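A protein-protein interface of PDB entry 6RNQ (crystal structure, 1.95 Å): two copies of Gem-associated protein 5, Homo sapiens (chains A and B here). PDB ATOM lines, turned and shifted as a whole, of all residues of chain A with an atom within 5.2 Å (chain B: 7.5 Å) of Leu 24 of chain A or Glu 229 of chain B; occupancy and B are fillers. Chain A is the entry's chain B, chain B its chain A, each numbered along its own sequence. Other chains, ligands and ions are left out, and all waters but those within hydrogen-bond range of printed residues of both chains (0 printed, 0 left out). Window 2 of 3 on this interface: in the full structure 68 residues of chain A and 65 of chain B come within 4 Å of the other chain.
The side-chain hydroxyl (OG) of Ser 223 of chain B sits close to a ring nitrogen (NE2) of His 20 of chain A (3.4 Å). OD2 of Asp 22 of chain A is in salt-bridge range of NZ of Lys 200 of chain B (2.9 Å).
The backbone carbonyl oxygen (O) of Leu 24 of chain A is in hydrogen-bond range of the side-chain hydroxyl (OG1) of Thr 28 of chain A, 3.0 Å away. O of Ala 222 of chain B sits at hydrogen-bond distance from OG1 of Thr 226 of chain B (3.2 Å). The backbone carbonyl oxygen (O) of Ser 223 of chain B sits at hydrogen-bond distance from the side-chain hydroxyl (OG1) of Thr 226 of chain B (3.1 Å). OE2 of Glu 229 of chain B is in salt-bridge range of NE of Arg 225 of chain B, 2.6 Å away.
No position is printed for both chains.
Of the printed residues of chain B, Asp 22 of chain A touches Lys 200. Of the printed residues of chain B, Cys 23 of chain A touches Lys 200 (3.9 Å) and Leu 203 (3.5 Å). Of the printed residues of chain B, Leu 24 of chain A touches Thr 226, Glu 229, Leu 230 and Ile 233. Printed residues of chain A within 4 Å of Thr 226 of chain B: His 20 and Leu 24. Glu 229 of chain B touches one residue of chain A. Ser 240 of chain B touches none of the printed residues of chain A. The nearest printed residue of chain B that does not touch Leu 24 of chain A is Leu 203 of chain B (5.5 Å). The nearest printed residue of chain A that does not touch Glu 229 of chain B is Ala 27 of chain A (6.4 Å).
His 20 of chain A touches Leu 215 of chain B. Ala 222 of chain B touches His 20 of chain A (C to CE1, 3.95 Å). CB of His 20 of chain A touches CG2 of Thr 226 of chain B, 3.6 Å away. Cys 23 of chain A touches Lys 200 of chain B. Leu 24 of chain A touches Glu 229 of chain B (CD1 to OE1, 3.4 Å). Leu 24 of chain A touches Leu 230 of chain B. Ile 233 of chain B touches Leu 24 of chain A. CD2 of Leu 26 of chain A touches CB of Leu 203 of chain B, 3.6 Å away. Ala 27 of chain A touches Leu 203 of chain B. Thr 28 of chain A touches Ile 233 of chain B.
Of the 10 printed residues of chain A, 7 touch a printed residue of chain B. Hydrophobic or aromatic side chains of chain A within 4 Å of the printed part of chain B: His 20, Leu 24, Leu 26 and Ala 27. Among the printed residues, 16 pairs touch across the chains. Among the printed residues, Asp or Glu carboxylates within 4 Å of a Lys or Arg side-chain nitrogen of the other chain: Asp 22 of chain A with Lys 200 of chain B.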
ATOM      1  N   HIS A  20      26.182   5.039 -13.132  1.00  0.00           N
ATOM      2  CA  HIS A  20      25.318   4.546 -12.044  1.00  0.00           C
ATOM      3  C   HIS A  20      24.247   5.593 -11.790  1.00  0.00           C
ATOM      4  O   HIS A  20      23.131   5.238 -11.776  1.00  0.00           O
ATOM      5  CB  HIS A  20      26.170   4.186 -10.834  1.00  0.00           C
ATOM      6  CG  HIS A  20      26.887   2.894 -10.978  1.00  0.00           C
ATOM      7  ND1 HIS A  20      27.836   2.490 -10.113  1.00  0.00           N
ATOM      8  CD2 HIS A  20      26.842   1.948 -11.918  1.00  0.00           C
ATOM      9  CE1 HIS A  20      28.322   1.347 -10.491  1.00  0.00           C
ATOM     10  NE2 HIS A  20      27.742   1.000 -11.584  1.00  0.00           N
ATOM     11  N   GLN A  21      24.599   6.869 -11.758  1.00  0.00           N
ATOM     12  CA  GLN A  21      23.635   7.974 -11.563  1.00  0.00           C
ATOM     13  C   GLN A  21      22.659   7.963 -12.733  1.00  0.00           C
ATOM     14  O   GLN A  21      21.498   8.127 -12.520  1.00  0.00           O
ATOM     15  CB  GLN A  21      24.331   9.324 -11.453  1.00  0.00           C
ATOM     16  CG  GLN A  21      24.663   9.737 -10.026  1.00  0.00           C
ATOM     17  CD  GLN A  21      25.701  10.832  -9.904  1.00  0.00           C
ATOM     18  OE1 GLN A  21      25.385  12.004  -9.752  1.00  0.00           O
ATOM     19  NE2 GLN A  21      26.965  10.460  -9.934  1.00  0.00           N
ATOM     20  N   ASP A  22      23.138   7.724 -13.937  1.00  0.00           N
ATOM     21  CA  ASP A  22      22.285   7.686 -15.138  1.00  0.00           C
ATOM     22  C   ASP A  22      21.229   6.614 -15.023  1.00  0.00           C
ATOM     23  O   ASP A  22      20.135   6.907 -15.286  1.00  0.00           O
ATOM     24  CB  ASP A  22      23.064   7.254 -16.360  1.00  0.00           C
ATOM     25  CG  ASP A  22      23.924   8.341 -16.915  1.00  0.00           C
ATOM     26  OD1 ASP A  22      23.785   9.456 -16.478  1.00  0.00           O
ATOM     27  OD2 ASP A  22      24.688   8.080 -17.824  1.00  0.00           O
ATOM     28  N   CYS A  23      21.577   5.425 -14.585  1.00  0.00           N
ATOM     29  CA  CYS A  23      20.634   4.302 -14.467  1.00  0.00           C
ATOM     30  C   CYS A  23      19.522   4.669 -13.499  1.00  0.00           C
ATOM     31  O   CYS A  23      18.419   4.390 -13.780  1.00  0.00           O
ATOM     32  CB  CYS A  23      21.332   3.056 -13.968  1.00  0.00           C
ATOM     33  SG  CYS A  23      22.482   2.331 -15.150  1.00  0.00           S
ATOM     34  N   LEU A  24      19.840   5.327 -12.407  1.00  0.00           N
ATOM     35  CA  LEU A  24      18.851   5.721 -11.386  1.00  0.00           C
ATOM     36  C   LEU A  24      17.920   6.773 -11.960  1.00  0.00           C
ATOM     37  O   LEU A  24      16.733   6.561 -11.922  1.00  0.00           O
ATOM     38  CB  LEU A  24      19.608   6.202 -10.157  1.00  0.00           C
ATOM     39  CG  LEU A  24      20.377   5.095  -9.463  1.00  0.00           C
ATOM     40  CD1 LEU A  24      20.917   5.560  -8.148  1.00  0.00           C
ATOM     41  CD2 LEU A  24      19.500   3.898  -9.276  1.00  0.00           C
ATOM     42  N   VAL A  25      18.452   7.865 -12.467  1.00  0.00           N
ATOM     43  CA  VAL A  25      17.617   8.890 -13.088  1.00  0.00           C
ATOM     44  C   VAL A  25      16.744   8.265 -14.170  1.00  0.00           C
ATOM     45  O   VAL A  25      15.538   8.519 -14.250  1.00  0.00           O
ATOM     46  CB  VAL A  25      18.487  10.027 -13.649  1.00  0.00           C
ATOM     47  CG1 VAL A  25      17.640  10.996 -14.462  1.00  0.00           C
ATOM     48  CG2 VAL A  25      19.202  10.753 -12.512  1.00  0.00           C
ATOM     49  N   LEU A  26      17.345   7.412 -15.006  1.00  0.00           N
ATOM     50  CA  LEU A  26      16.602   6.784 -16.093  1.00  0.00           C
ATOM     51  C   LEU A  26      15.505   5.872 -15.562  1.00  0.00           C
ATOM     52  O   LEU A  26      14.393   5.842 -16.104  1.00  0.00           O
ATOM     53  CB  LEU A  26      17.562   6.001 -16.988  1.00  0.00           C
ATOM     54  CG  LEU A  26      16.958   5.315 -18.213  1.00  0.00           C
ATOM     55  CD1 LEU A  26      16.379   6.344 -19.167  1.00  0.00           C
ATOM     56  CD2 LEU A  26      18.008   4.465 -18.905  1.00  0.00           C
ATOM     57  N   ALA A  27      15.799   5.107 -14.506  1.00  0.00           N
ATOM     58  CA  ALA A  27      14.779   4.244 -13.919  1.00  0.00           C
ATOM     59  C   ALA A  27      13.654   5.069 -13.311  1.00  0.00           C
ATOM     60  O   ALA A  27      12.476   4.714 -13.441  1.00  0.00           O
ATOM     61  CB  ALA A  27      15.405   3.329 -12.867  1.00  0.00           C
ATOM     62  N   THR A  28      13.996   6.176 -12.648  1.00  0.00           N
ATOM     63  CA  THR A  28      12.975   7.047 -12.076  1.00  0.00           C
ATOM     64  C   THR A  28      12.072   7.618 -13.164  1.00  0.00           C
ATOM     65  O   THR A  28      10.843   7.631 -13.026  1.00  0.00           O
ATOM     66  CB  THR A  28      13.638   8.173 -11.281  1.00  0.00           C
ATOM     67  OG1 THR A  28      14.455   7.618 -10.241  1.00  0.00           O
ATOM     68  CG2 THR A  28      12.591   9.091 -10.664  1.00  0.00           C
ATOM     69  N   ALA A  29      12.667   8.091 -14.263  1.00  0.00           N
ATOM     70  CA  ALA A  29      11.886   8.724 -15.320  1.00  0.00           C
ATOM     71  C   ALA A  29      10.957   7.725 -15.998  1.00  0.00           C
ATOM     72  O   ALA A  29       9.760   7.988 -16.161  1.00  0.00           O
ATOM     73  CB  ALA A  29      12.820   9.370 -16.344  1.00  0.00           C
ATOM     74  N   LYS B 200      21.204   0.450 -18.913  1.00  0.00           N
ATOM     75  CA  LYS B 200      20.517   1.567 -19.555  1.00  0.00           C
ATOM     76  C   LYS B 200      19.682   1.098 -20.747  1.00  0.00           C
ATOM     77  O   LYS B 200      18.535   1.530 -20.919  1.00  0.00           O
ATOM     78  CB  LYS B 200      21.526   2.627 -19.999  1.00  0.00           C
ATOM     79  CG  LYS B 200      22.029   3.525 -18.865  1.00  0.00           C
ATOM     80  CD  LYS B 200      22.273   4.953 -19.380  1.00  0.00           C
ATOM     81  CE  LYS B 200      23.675   5.148 -19.908  1.00  0.00           C
ATOM     82  NZ  LYS B 200      23.938   6.569 -20.208  1.00  0.00           N
ATOM     83  N   LEU B 203      16.614  -0.714 -19.400  1.00  0.00           N
ATOM     84  CA  LEU B 203      15.646   0.293 -18.962  1.00  0.00           C
ATOM     85  C   LEU B 203      14.918   0.918 -20.150  1.00  0.00           C
ATOM     86  O   LEU B 203      13.716   1.202 -20.076  1.00  0.00           O
ATOM     87  CB  LEU B 203      16.354   1.374 -18.138  1.00  0.00           C
ATOM     88  CG  LEU B 203      16.810   0.934 -16.736  1.00  0.00           C
ATOM     89  CD1 LEU B 203      17.775   1.912 -16.127  1.00  0.00           C
ATOM     90  CD2 LEU B 203      15.598   0.781 -15.841  1.00  0.00           C
ATOM     91  N   ALA B 212      18.434  -4.145 -13.390  1.00  0.00           N
ATOM     92  CA  ALA B 212      19.024  -4.359 -12.074  1.00  0.00           C
ATOM     93  C   ALA B 212      19.963  -5.557 -12.098  1.00  0.00           C
ATOM     94  O   ALA B 212      21.133  -5.457 -11.713  1.00  0.00           O
ATOM     95  CB  ALA B 212      17.922  -4.558 -11.035  1.00  0.00           C
ATOM     96  N   LEU B 215      23.228  -4.991 -14.048  1.00  0.00           N
ATOM     97  CA  LEU B 215      24.100  -4.084 -13.310  1.00  0.00           C
ATOM     98  C   LEU B 215      24.757  -4.799 -12.131  1.00  0.00           C
ATOM     99  O   LEU B 215      25.862  -4.430 -11.715  1.00  0.00           O
ATOM    100  CB  LEU B 215      23.292  -2.876 -12.851  1.00  0.00           C
ATOM    101  CG  LEU B 215      24.047  -1.720 -12.220  1.00  0.00           C
ATOM    102  CD1 LEU B 215      25.149  -1.206 -13.095  1.00  0.00           C
ATOM    103  CD2 LEU B 215      23.053  -0.597 -11.897  1.00  0.00           C
ATOM    104  N   ALA B 222      29.568  -0.943  -5.360  1.00  0.00           N
ATOM    105  CA  ALA B 222      28.864   0.184  -5.960  1.00  0.00           C
ATOM    106  C   ALA B 222      27.790  -0.288  -6.933  1.00  0.00           C
ATOM    107  O   ALA B 222      26.664   0.226  -6.927  1.00  0.00           O
ATOM    108  CB  ALA B 222      29.858   1.099  -6.671  1.00  0.00           C
ATOM    109  N   SER B 223      28.116  -1.271  -7.772  1.00  0.00           N
ATOM    110  CA  SER B 223      27.154  -1.758  -8.755  1.00  0.00           C
ATOM    111  C   SER B 223      26.014  -2.507  -8.074  1.00  0.00           C
ATOM    112  O   SER B 223      24.838  -2.287  -8.388  1.00  0.00           O
ATOM    113  CB  SER B 223      27.866  -2.647  -9.777  1.00  0.00           C
ATOM    114  OG  SER B 223      28.945  -1.940 -10.389  1.00  0.00           O
ATOM    115  N   LEU B 224      26.342  -3.399  -7.139  1.00  0.00           N
ATOM    116  CA  LEU B 224      25.300  -4.077  -6.378  1.00  0.00           C
ATOM    117  C   LEU B 224      24.405  -3.068  -5.675  1.00  0.00           C
ATOM    118  O   LEU B 224      23.176  -3.195  -5.699  1.00  0.00           O
ATOM    119  CB  LEU B 224      25.938  -5.041  -5.386  1.00  0.00           C
ATOM    120  CG  LEU B 224      26.605  -6.274  -5.995  1.00  0.00           C
ATOM    121  CD1 LEU B 224      27.510  -6.969  -4.981  1.00  0.00           C
ATOM    122  CD2 LEU B 224      25.553  -7.244  -6.512  1.00  0.00           C
ATOM    123  N   ARG B 225      24.999  -2.039  -5.071  1.00  0.00           N
ATOM    124  CA  ARG B 225      24.216  -1.001  -4.408  1.00  0.00           C
ATOM    125  C   ARG B 225      23.256  -0.320  -5.390  1.00  0.00           C
ATOM    126  O   ARG B 225      22.032  -0.331  -5.204  1.00  0.00           O
ATOM    127  CB  ARG B 225      25.166   0.020  -3.771  1.00  0.00           C
ATOM    128  CG  ARG B 225      24.466   1.229  -3.177  1.00  0.00           C
ATOM    129  CD  ARG B 225      23.308   0.780  -2.326  1.00  0.00           C
ATOM    130  NE  ARG B 225      22.624   1.896  -1.680  1.00  0.00           N
ATOM    131  CZ  ARG B 225      22.915   2.350  -0.458  1.00  0.00           C
ATOM    132  NH1 ARG B 225      23.893   1.794   0.257  1.00  0.00           N
ATOM    133  NH2 ARG B 225      22.231   3.369   0.047  1.00  0.00           N
ATOM    134  N   THR B 226      23.794   0.293  -6.446  1.00  0.00           N
ATOM    135  CA  THR B 226      22.921   1.006  -7.378  1.00  0.00           C
ATOM    136  C   THR B 226      21.875   0.076  -7.989  1.00  0.00           C
ATOM    137  O   THR B 226      20.737   0.493  -8.220  1.00  0.00           O
ATOM    138  CB  THR B 226      23.754   1.682  -8.465  1.00  0.00           C
ATOM    139  OG1 THR B 226      24.482   0.697  -9.206  1.00  0.00           O
ATOM    140  CG2 THR B 226      24.722   2.691  -7.850  1.00  0.00           C
ATOM    141  N   ALA B 227      22.227  -1.188  -8.241  1.00  0.00           N
ATOM    142  CA  ALA B 227      21.241  -2.145  -8.739  1.00  0.00           C
ATOM    143  C   ALA B 227      20.101  -2.346  -7.744  1.00  0.00           C
ATOM    144  O   ALA B 227      18.927  -2.422  -8.138  1.00  0.00           O
ATOM    145  CB  ALA B 227      21.920  -3.477  -9.046  1.00  0.00           C
ATOM    146  N   ALA B 228      20.424  -2.453  -6.448  1.00  0.00           N
ATOM    147  CA  ALA B 228      19.380  -2.621  -5.442  1.00  0.00           C
ATOM    148  C   ALA B 228      18.474  -1.397  -5.389  1.00  0.00           C
ATOM    149  O   ALA B 228      17.248  -1.526  -5.278  1.00  0.00           O
ATOM    150  CB  ALA B 228      20.008  -2.888  -4.067  1.00  0.00           C
ATOM    151  N   GLU B 229      19.059  -0.197  -5.450  1.00  0.00           N
ATOM    152  CA  GLU B 229      18.250   1.017  -5.501  1.00  0.00           C
ATOM    153  C   GLU B 229      17.413   1.074  -6.776  1.00  0.00           C
ATOM    154  O   GLU B 229      16.297   1.608  -6.773  1.00  0.00           O
ATOM    155  CB  GLU B 229      19.150   2.247  -5.405  1.00  0.00           C
ATOM    156  CG  GLU B 229      19.726   2.477  -4.036  1.00  0.00           C
ATOM    157  CD  GLU B 229      20.846   3.505  -4.028  1.00  0.00           C
ATOM    158  OE1 GLU B 229      21.209   4.002  -5.120  1.00  0.00           O
ATOM    159  OE2 GLU B 229      21.362   3.809  -2.916  1.00  0.00           O
ATOM    160  N   LEU B 230      17.920   0.521  -7.873  1.00  0.00           N
ATOM    161  CA  LEU B 230      17.153   0.509  -9.115  1.00  0.00           C
ATOM    162  C   LEU B 230      15.931  -0.392  -8.992  1.00  0.00           C
ATOM    163  O   LEU B 230      14.834  -0.029  -9.435  1.00  0.00           O
ATOM    164  CB  LEU B 230      18.050   0.053 -10.263  1.00  0.00           C
ATOM    165  CG  LEU B 230      17.612   0.365 -11.688  1.00  0.00           C
ATOM    166  CD1 LEU B 230      18.763   0.053 -12.661  1.00  0.00           C
ATOM    167  CD2 LEU B 230      16.366  -0.404 -12.060  1.00  0.00           C
ATOM    168  N   ALA B 231      16.100  -1.574  -8.391  1.00  0.00           N
ATOM    169  CA  ALA B 231      14.963  -2.468  -8.197  1.00  0.00           C
ATOM    170  C   ALA B 231      13.931  -1.844  -7.266  1.00  0.00           C
ATOM    171  O   ALA B 231      12.721  -2.014  -7.465  1.00  0.00           O
ATOM    172  CB  ALA B 231      15.440  -3.814  -7.655  1.00  0.00           C
ATOM    173  N   ALA B 232      14.386  -1.107  -6.250  1.00  0.00           N
ATOM    174  CA  ALA B 232      13.456  -0.452  -5.333  1.00  0.00           C
ATOM    175  C   ALA B 232      12.634   0.615  -6.053  1.00  0.00           C
ATOM    176  O   ALA B 232      11.413   0.713  -5.866  1.00  0.00           O
ATOM    177  CB  ALA B 232      14.223   0.163  -4.159  1.00  0.00           C
ATOM    178  N   ILE B 233      13.287   1.419  -6.893  1.00  0.00           N
ATOM    179  CA  ILE B 233      12.578   2.471  -7.620  1.00  0.00           C
ATOM    180  C   ILE B 233      11.442   1.879  -8.442  1.00  0.00           C
ATOM    181  O   ILE B 233      10.365   2.471  -8.553  1.00  0.00           O
ATOM    182  CB  ILE B 233      13.568   3.262  -8.490  1.00  0.00           C
ATOM    183  CG1 ILE B 233      14.531   4.045  -7.592  1.00  0.00           C
ATOM    184  CG2 ILE B 233      12.826   4.189  -9.441  1.00  0.00           C
ATOM    185  CD1 ILE B 233      15.809   4.445  -8.285  1.00  0.00           C
ATOM    186  N   VAL B 234      11.649   0.688  -8.998  1.00  0.00           N
ATOM    187  CA  VAL B 234      10.647   0.050  -9.847  1.00  0.00           C
ATOM    188  C   VAL B 234       9.654  -0.794  -9.072  1.00  0.00           C
ATOM    189  O   VAL B 234       8.685  -1.289  -9.664  1.00  0.00           O
ATOM    190  CB  VAL B 234      11.371  -0.801 -10.911  1.00  0.00           C
ATOM    191  CG1 VAL B 234      10.387  -1.635 -11.715  1.00  0.00           C
ATOM    192  CG2 VAL B 234      12.179   0.110 -11.845  1.00  0.00           C
ATOM    193  N   GLY B 235       9.835  -0.948  -7.771  1.00  0.00           N
ATOM    194  CA  GLY B 235       8.932  -1.745  -6.979  1.00  0.00           C
ATOM    195  C   GLY B 235       9.255  -3.219  -6.930  1.00  0.00           C
ATOM    196  O   GLY B 235       8.395  -4.011  -6.516  1.00  0.00           O
ATOM    197  N   SER B 240      15.395  -6.137  -4.729  1.00  0.00           N
ATOM    198  CA  SER B 240      16.206  -5.094  -4.107  1.00  0.00           C
ATOM    199  C   SER B 240      16.865  -5.599  -2.827  1.00  0.00           C
ATOM    200  O   SER B 240      18.069  -5.406  -2.614  1.00  0.00           O
ATOM    201  CB  SER B 240      15.339  -3.873  -3.819  1.00  0.00           C
ATOM    202  OG  SER B 240      16.107  -2.847  -3.219  1.00  0.00           O
ATOM    203  N   LEU B 243      19.727  -7.989  -3.606  1.00  0.00           N
ATOM    204  CA  LEU B 243      20.924  -7.307  -4.085  1.00  0.00           C
ATOM    205  C   LEU B 243      21.557  -6.448  -2.994  1.00  0.00           C
ATOM    206  O   LEU B 243      22.787  -6.342  -2.915  1.00  0.00           O
ATOM    207  CB  LEU B 243      20.585  -6.448  -5.298  1.00  0.00           C
ATOM    208  CG  LEU B 243      20.038  -7.184  -6.525  1.00  0.00           C
ATOM    209  CD1 LEU B 243      19.673  -6.163  -7.587  1.00  0.00           C
ATOM    210  CD2 LEU B 243      21.034  -8.188  -7.046  1.00  0.00           C
ATOM    211  N   ALA B 244      20.738  -5.797  -2.164  1.00  0.00           N
ATOM    212  CA  ALA B 244      21.293  -4.966  -1.096  1.00  0.00           C
ATOM    213  C   ALA B 244      22.046  -5.800  -0.063  1.00  0.00           C
ATOM    214  O   ALA B 244      23.022  -5.319   0.531  1.00  0.00           O
ATOM    215  CB  ALA B 244      20.180  -4.164  -0.421  1.00  0.00           C
